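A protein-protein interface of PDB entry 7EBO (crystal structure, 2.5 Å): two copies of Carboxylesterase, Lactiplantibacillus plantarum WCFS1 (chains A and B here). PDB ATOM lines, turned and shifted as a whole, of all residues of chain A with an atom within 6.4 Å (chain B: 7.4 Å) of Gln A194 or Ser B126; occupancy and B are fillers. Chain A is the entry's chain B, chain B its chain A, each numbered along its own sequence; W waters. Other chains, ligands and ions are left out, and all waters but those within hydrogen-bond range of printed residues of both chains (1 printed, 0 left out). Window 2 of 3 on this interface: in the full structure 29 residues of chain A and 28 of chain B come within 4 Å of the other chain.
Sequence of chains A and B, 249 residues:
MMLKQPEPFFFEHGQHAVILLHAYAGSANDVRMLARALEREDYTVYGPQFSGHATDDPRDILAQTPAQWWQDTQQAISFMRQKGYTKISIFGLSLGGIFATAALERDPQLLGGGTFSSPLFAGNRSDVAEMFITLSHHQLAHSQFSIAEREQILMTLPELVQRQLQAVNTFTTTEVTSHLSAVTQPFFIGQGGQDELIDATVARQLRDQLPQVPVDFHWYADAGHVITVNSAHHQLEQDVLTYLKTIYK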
ATOM      1  N   GLY A 192     -15.554  16.191   3.194  1.00  0.00           N
ATOM      2  CA  GLY A 192     -15.543  17.120   4.304  1.00  0.00           C
ATOM      3  C   GLY A 192     -14.119  17.309   4.786  1.00  0.00           C
ATOM      4  O   GLY A 192     -13.346  16.349   4.873  1.00  0.00           O
ATOM      5  N   GLY A 193     -13.783  18.555   5.132  1.00  0.00           N
ATOM      6  CA  GLY A 193     -12.421  18.872   5.526  1.00  0.00           C
ATOM      7  C   GLY A 193     -12.043  18.354   6.898  1.00  0.00           C
ATOM      8  O   GLY A 193     -10.871  18.062   7.151  1.00  0.00           O
ATOM      9  N   GLN A 194     -13.018  18.236   7.796  1.00  0.00           N
ATOM     10  CA  GLN A 194     -12.788  17.777   9.157  1.00  0.00           C
ATOM     11  C   GLN A 194     -13.016  16.275   9.303  1.00  0.00           C
ATOM     12  O   GLN A 194     -13.219  15.795  10.424  1.00  0.00           O
ATOM     13  CB  GLN A 194     -13.698  18.535  10.130  1.00  0.00           C
ATOM     14  CG  GLN A 194     -13.734  20.051   9.939  1.00  0.00           C
ATOM     15  CD  GLN A 194     -12.562  20.767  10.582  1.00  0.00           C
ATOM     16  OE1 GLN A 194     -11.892  20.222  11.456  1.00  0.00           O
ATOM     17  NE2 GLN A 194     -12.314  22.001  10.153  1.00  0.00           N
ATOM     18  N   ASP A 195     -12.988  15.533   8.194  1.00  0.00           N
ATOM     19  CA  ASP A 195     -13.340  14.116   8.206  1.00  0.00           C
ATOM     20  C   ASP A 195     -12.477  13.327   9.182  1.00  0.00           C
ATOM     21  O   ASP A 195     -11.259  13.212   9.014  1.00  0.00           O
ATOM     22  CB  ASP A 195     -13.211  13.534   6.797  1.00  0.00           C
ATOM     23  CG  ASP A 195     -13.804  12.133   6.675  1.00  0.00           C
ATOM     24  OD1 ASP A 195     -13.767  11.353   7.652  1.00  0.00           O
ATOM     25  OD2 ASP A 195     -14.317  11.811   5.585  1.00  0.00           O
ATOM     26  N   GLU A 196     -13.136  12.790  10.207  1.00  0.00           N
ATOM     27  CA  GLU A 196     -12.502  11.968  11.227  1.00  0.00           C
ATOM     28  C   GLU A 196     -12.342  10.526  10.767  1.00  0.00           C
ATOM     29  O   GLU A 196     -11.333   9.879  11.069  1.00  0.00           O
ATOM     30  CB  GLU A 196     -13.329  12.011  12.514  1.00  0.00           C
ATOM     31  CG  GLU A 196     -14.596  12.861  12.426  1.00  0.00           C
ATOM     32  CD  GLU A 196     -15.653  12.307  11.474  1.00  0.00           C
ATOM     33  OE1 GLU A 196     -16.314  11.304  11.815  1.00  0.00           O
ATOM     34  OE2 GLU A 196     -15.810  12.882  10.375  1.00  0.00           O
ATOM     35  N   LEU A 197     -13.336  10.015  10.040  1.00  0.00           N
ATOM     36  CA  LEU A 197     -13.378   8.595   9.714  1.00  0.00           C
ATOM     37  C   LEU A 197     -12.292   8.199   8.722  1.00  0.00           C
ATOM     38  O   LEU A 197     -11.607   7.187   8.910  1.00  0.00           O
ATOM     39  CB  LEU A 197     -14.762   8.265   9.151  1.00  0.00           C
ATOM     40  CG  LEU A 197     -15.458   6.951   9.483  1.00  0.00           C
ATOM     41  CD1 LEU A 197     -15.312   6.641  10.956  1.00  0.00           C
ATOM     42  CD2 LEU A 197     -16.927   7.062   9.104  1.00  0.00           C
ATOM     43  N   ALA A 200      -8.862  12.652   4.594  1.00  0.00           N
ATOM     44  CA  ALA A 200      -9.559  13.638   3.769  1.00  0.00           C
ATOM     45  C   ALA A 200      -8.862  13.877   2.434  1.00  0.00           C
ATOM     46  O   ALA A 200      -9.526  14.166   1.432  1.00  0.00           O
ATOM     47  CB  ALA A 200      -9.699  14.953   4.537  1.00  0.00           C
ATOM     48  N   TYR A 220     -15.785  20.505   1.839  1.00  0.00           N
ATOM     49  CA  TYR A 220     -16.652  21.020   2.886  1.00  0.00           C
ATOM     50  C   TYR A 220     -15.749  21.101   4.111  1.00  0.00           C
ATOM     51  O   TYR A 220     -15.710  20.200   4.951  1.00  0.00           O
ATOM     52  CB  TYR A 220     -17.881  20.153   3.038  1.00  0.00           C
ATOM     53  CG  TYR A 220     -18.585  20.049   1.704  1.00  0.00           C
ATOM     54  CD1 TYR A 220     -18.367  18.974   0.855  1.00  0.00           C
ATOM     55  CD2 TYR A 220     -19.420  21.070   1.266  1.00  0.00           C
ATOM     56  CE1 TYR A 220     -18.988  18.901  -0.379  1.00  0.00           C
ATOM     57  CE2 TYR A 220     -20.042  21.007   0.038  1.00  0.00           C
ATOM     58  CZ  TYR A 220     -19.825  19.921  -0.780  1.00  0.00           C
ATOM     59  OH  TYR A 220     -20.445  19.855  -2.004  1.00  0.00           O
ATOM     60  N   ALA A 221     -15.028  22.221   4.192  1.00  0.00           N
ATOM     61  CA  ALA A 221     -13.886  22.346   5.090  1.00  0.00           C
ATOM     62  C   ALA A 221     -14.288  22.263   6.551  1.00  0.00           C
ATOM     63  O   ALA A 221     -13.501  21.803   7.386  1.00  0.00           O
ATOM     64  CB  ALA A 221     -13.161  23.661   4.810  1.00  0.00           C
ATOM     65  N   ASP A 222     -15.488  22.721   6.882  1.00  0.00           N
ATOM     66  CA  ASP A 222     -15.968  22.772   8.253  1.00  0.00           C
ATOM     67  C   ASP A 222     -16.692  21.503   8.688  1.00  0.00           C
ATOM     68  O   ASP A 222     -17.202  21.458   9.811  1.00  0.00           O
ATOM     69  CB  ASP A 222     -16.903  23.971   8.418  1.00  0.00           C
ATOM     70  CG  ASP A 222     -18.225  23.772   7.703  1.00  0.00           C
ATOM     71  OD1 ASP A 222     -19.253  23.608   8.391  1.00  0.00           O
ATOM     72  OD2 ASP A 222     -18.232  23.749   6.453  1.00  0.00           O
ATOM     73  N   ALA A 223     -16.733  20.468   7.852  1.00  0.00           N
ATOM     74  CA  ALA A 223     -17.617  19.340   8.097  1.00  0.00           C
ATOM     75  C   ALA A 223     -16.876  18.020   8.265  1.00  0.00           C
ATOM     76  O   ALA A 223     -15.766  17.832   7.759  1.00  0.00           O
ATOM     77  CB  ALA A 223     -18.631  19.195   6.958  1.00  0.00           C
ATOM     78  N   GLY A 224     -17.535  17.109   8.976  1.00  0.00           N
ATOM     79  CA  GLY A 224     -17.093  15.742   9.142  1.00  0.00           C
ATOM     80  C   GLY A 224     -17.436  14.883   7.938  1.00  0.00           C
ATOM     81  O   GLY A 224     -17.805  15.365   6.866  1.00  0.00           O
ATOM     82  N   HIS A 225     -17.314  13.567   8.139  1.00  0.00           N
ATOM     83  CA  HIS A 225     -17.371  12.624   7.025  1.00  0.00           C
ATOM     84  C   HIS A 225     -18.740  12.605   6.351  1.00  0.00           C
ATOM     85  O   HIS A 225     -18.835  12.712   5.123  1.00  0.00           O
ATOM     86  CB  HIS A 225     -17.012  11.222   7.515  1.00  0.00           C
ATOM     87  CG  HIS A 225     -17.407  10.137   6.561  1.00  0.00           C
ATOM     88  ND1 HIS A 225     -16.731   9.901   5.384  1.00  0.00           N
ATOM     89  CD2 HIS A 225     -18.423   9.243   6.596  1.00  0.00           C
ATOM     90  CE1 HIS A 225     -17.304   8.899   4.742  1.00  0.00           C
ATOM     91  NE2 HIS A 225     -18.335   8.482   5.456  1.00  0.00           N
ATOM     92  N   GLY B 123      -7.196  20.163  24.347  1.00  0.00           N
ATOM     93  CA  GLY B 123      -6.832  20.565  23.010  1.00  0.00           C
ATOM     94  C   GLY B 123      -7.996  20.462  22.057  1.00  0.00           C
ATOM     95  O   GLY B 123      -9.154  20.400  22.470  1.00  0.00           O
ATOM     96  N   ASN B 124      -7.663  20.444  20.770  1.00  0.00           N
ATOM     97  CA  ASN B 124      -8.674  20.358  19.726  1.00  0.00           C
ATOM     98  C   ASN B 124      -9.398  19.020  19.815  1.00  0.00           C
ATOM     99  O   ASN B 124      -8.770  17.959  19.737  1.00  0.00           O
ATOM    100  CB  ASN B 124      -8.026  20.537  18.356  1.00  0.00           C
ATOM    101  CG  ASN B 124      -9.031  20.878  17.278  1.00  0.00           C
ATOM    102  OD1 ASN B 124     -10.152  20.380  17.283  1.00  0.00           O
ATOM    103  ND2 ASN B 124      -8.636  21.745  16.352  1.00  0.00           N
ATOM    104  N   ARG B 125     -10.719  19.073  19.991  1.00  0.00           N
ATOM    105  CA  ARG B 125     -11.556  17.880  20.033  1.00  0.00           C
ATOM    106  C   ARG B 125     -12.502  17.809  18.837  1.00  0.00           C
ATOM    107  O   ARG B 125     -13.501  17.085  18.882  1.00  0.00           O
ATOM    108  CB  ARG B 125     -12.339  17.824  21.348  1.00  0.00           C
ATOM    109  CG  ARG B 125     -12.044  16.590  22.187  1.00  0.00           C
ATOM    110  CD  ARG B 125     -10.572  16.234  22.098  1.00  0.00           C
ATOM    111  NE  ARG B 125      -9.858  16.411  23.358  1.00  0.00           N
ATOM    112  CZ  ARG B 125      -8.547  16.617  23.438  1.00  0.00           C
ATOM    113  NH1 ARG B 125      -7.822  16.690  22.330  1.00  0.00           N
ATOM    114  NH2 ARG B 125      -7.962  16.763  24.620  1.00  0.00           N
ATOM    115  N   SER B 126     -12.191  18.537  17.758  1.00  0.00           N
ATOM    116  CA  SER B 126     -13.050  18.575  16.577  1.00  0.00           C
ATOM    117  C   SER B 126     -13.226  17.217  15.918  1.00  0.00           C
ATOM    118  O   SER B 126     -14.172  17.034  15.142  1.00  0.00           O
ATOM    119  CB  SER B 126     -12.485  19.547  15.542  1.00  0.00           C
ATOM    120  OG  SER B 126     -13.101  19.349  14.283  1.00  0.00           O
ATOM    121  N   ASP B 127     -12.386  16.239  16.251  1.00  0.00           N
ATOM    122  CA  ASP B 127     -12.544  14.924  15.646  1.00  0.00           C
ATOM    123  C   ASP B 127     -13.572  14.107  16.406  1.00  0.00           C
ATOM    124  O   ASP B 127     -14.349  13.360  15.802  1.00  0.00           O
ATOM    125  CB  ASP B 127     -11.196  14.202  15.620  1.00  0.00           C
ATOM    126  CG  ASP B 127     -10.277  14.642  16.749  1.00  0.00           C
ATOM    127  OD1 ASP B 127     -10.066  15.864  16.902  1.00  0.00           O
ATOM    128  OD2 ASP B 127      -9.788  13.773  17.500  1.00  0.00           O
ATOM    129  N   VAL B 128     -13.608  14.255  17.730  1.00  0.00           N
ATOM    130  CA  VAL B 128     -14.604  13.540  18.513  1.00  0.00           C
ATOM    131  C   VAL B 128     -15.985  14.125  18.255  1.00  0.00           C
ATOM    132  O   VAL B 128     -16.988  13.401  18.256  1.00  0.00           O
ATOM    133  CB  VAL B 128     -14.228  13.570  20.007  1.00  0.00           C
ATOM    134  CG1 VAL B 128     -15.167  12.689  20.806  1.00  0.00           C
ATOM    135  CG2 VAL B 128     -12.784  13.121  20.194  1.00  0.00           C
ATOM    136  N   ALA B 129     -16.062  15.437  18.019  1.00  0.00           N
ATOM    137  CA  ALA B 129     -17.353  16.075  17.788  1.00  0.00           C
ATOM    138  C   ALA B 129     -18.006  15.572  16.505  1.00  0.00           C
ATOM    139  O   ALA B 129     -19.206  15.275  16.487  1.00  0.00           O
ATOM    140  CB  ALA B 129     -17.177  17.592  17.732  1.00  0.00           C
ATOM    141  N   GLU B 130     -17.236  15.481  15.419  1.00  0.00           N
ATOM    142  CA  GLU B 130     -17.792  15.000  14.160  1.00  0.00           C
ATOM    143  C   GLU B 130     -18.062  13.503  14.197  1.00  0.00           C
ATOM    144  O   GLU B 130     -19.020  13.030  13.575  1.00  0.00           O
ATOM    145  CB  GLU B 130     -16.857  15.355  13.009  1.00  0.00           C
ATOM    146  CG  GLU B 130     -16.741  16.841  12.752  1.00  0.00           C
ATOM    147  CD  GLU B 130     -18.044  17.437  12.258  1.00  0.00           C
ATOM    148  OE1 GLU B 130     -18.879  16.685  11.710  1.00  0.00           O
ATOM    149  OE2 GLU B 130     -18.237  18.659  12.420  1.00  0.00           O
ATOM    150  N   MET B 131     -17.226  12.744  14.909  1.00  0.00           N
ATOM    151  CA  MET B 131     -17.475  11.316  15.067  1.00  0.00           C
ATOM    152  C   MET B 131     -18.797  11.074  15.782  1.00  0.00           C
ATOM    153  O   MET B 131     -19.548  10.158  15.427  1.00  0.00           O
ATOM    154  CB  MET B 131     -16.323  10.663  15.829  1.00  0.00           C
ATOM    155  N   PHE B 132     -19.088  11.884  16.801  1.00  0.00           N
ATOM    156  CA  PHE B 132     -20.330  11.740  17.549  1.00  0.00           C
ATOM    157  C   PHE B 132     -21.535  11.978  16.645  1.00  0.00           C
ATOM    158  O   PHE B 132     -22.555  11.290  16.764  1.00  0.00           O
ATOM    159  CB  PHE B 132     -20.321  12.710  18.734  1.00  0.00           C
ATOM    160  CG  PHE B 132     -21.577  12.695  19.560  1.00  0.00           C
ATOM    161  CD1 PHE B 132     -21.671  11.865  20.663  1.00  0.00           C
ATOM    162  CD2 PHE B 132     -22.647  13.517  19.262  1.00  0.00           C
ATOM    163  CE1 PHE B 132     -22.810  11.842  21.445  1.00  0.00           C
ATOM    164  CE2 PHE B 132     -23.790  13.502  20.042  1.00  0.00           C
ATOM    165  CZ  PHE B 132     -23.872  12.662  21.134  1.00  0.00           C
ATOM    166  N   GLN B 162     -19.957  20.597  21.177  1.00  0.00           N
ATOM    167  CA  GLN B 162     -18.795  21.468  21.323  1.00  0.00           C
ATOM    168  C   GLN B 162     -18.686  21.995  22.746  1.00  0.00           C
ATOM    169  O   GLN B 162     -17.584  22.093  23.297  1.00  0.00           O
ATOM    170  CB  GLN B 162     -18.872  22.624  20.328  1.00  0.00           C
ATOM    171  CG  GLN B 162     -18.470  22.241  18.918  1.00  0.00           C
ATOM    172  CD  GLN B 162     -18.702  23.362  17.935  1.00  0.00           C
ATOM    173  OE1 GLN B 162     -19.013  24.486  18.327  1.00  0.00           O
ATOM    174  NE2 GLN B 162     -18.562  23.065  16.650  1.00  0.00           N
ATOM    175  N   LEU B 165     -17.593  18.865  25.105  1.00  0.00           N
ATOM    176  CA  LEU B 165     -16.180  18.553  24.911  1.00  0.00           C
ATOM    177  C   LEU B 165     -15.303  19.672  25.450  1.00  0.00           C
ATOM    178  O   LEU B 165     -14.186  19.425  25.922  1.00  0.00           O
ATOM    179  CB  LEU B 165     -15.885  18.320  23.430  1.00  0.00           C
ATOM    180  CG  LEU B 165     -16.463  17.058  22.791  1.00  0.00           C
ATOM    181  CD1 LEU B 165     -16.164  17.037  21.301  1.00  0.00           C
ATOM    182  CD2 LEU B 165     -15.912  15.821  23.471  1.00  0.00           C
HETATM  183  O   HOH W   1     -19.812  18.970  10.377  1.00  0.00           O
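OG of Ser B126 lies within hydrogen-bond range of OE1 of Gln A194 (3.2 Å). OE1 of Glu B130 lies within hydrogen-bond range of N of Gly A224 (3.1 Å).
The backbone carbonyl oxygen of Ala A223 lies within hydrogen-bond range of the backbone NH of Gln A194, 2.8 Å away. The backbone NH (N) of His A225 lies within hydrogen-bond range of the side-chain carboxylate (OE2) of Glu A196 (2.8 Å). The side-chain amide oxygen of Asn B124 is in hydrogen-bond range of the backbone NH of Ser B126 (2.8 Å). NE2 of Gln A194 lies within hydrogen-bond range of O of Ala A221, 3.0 Å away.
Among the printed residues, pairs that only touch across the chains: Glu A196 with Glu B130 (3.4 Å), Glu A196 with Asp B127 (3.4 Å), Glu A196 with Met B131 (3.5 Å) and Asp A222 with Glu B130 (3.96 Å).
Gln A194 touches just one residue of chain B: Ser B126 (3.2 Å). Of the printed residues of chain A, Ser B126 touches Gln A194 (3.2 Å). No residue of chain B comes within 4 Å of Gly A193. Of the printed residues of chain B, Gly A224 touches Glu B130. Of the printed residues of chain A, Glu B130 touches Glu A196, Asp A222 and Gly A224. Of the printed residues of chain A, Asp B127 touches Glu A196 (3.4 Å). Printed residues of chain B within 4 Å of Asp A222: Glu B130 (3.96 Å). Ala A200 touches none of the printed residues of chain B.
Of the 12 printed residues of chain B, 4 touch a printed residue of chain A. Printed residues of chain B that touch a printed residue of chain A: Ser B126, Asp B127, Glu B130 and Met B131. Along chain B the printed residues that touch a printed residue of chain A span positions 126 to 131. Of the 13 printed residues of chain A, 4 touch a printed residue of chain B.
No position is printed for both chains. Of the 6 pairs that touch across the chains among the printed residues, none has its exchanged pair printed and touching as well.
Water W1 bridges OE2 of Glu B130 and N of Gly A224.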
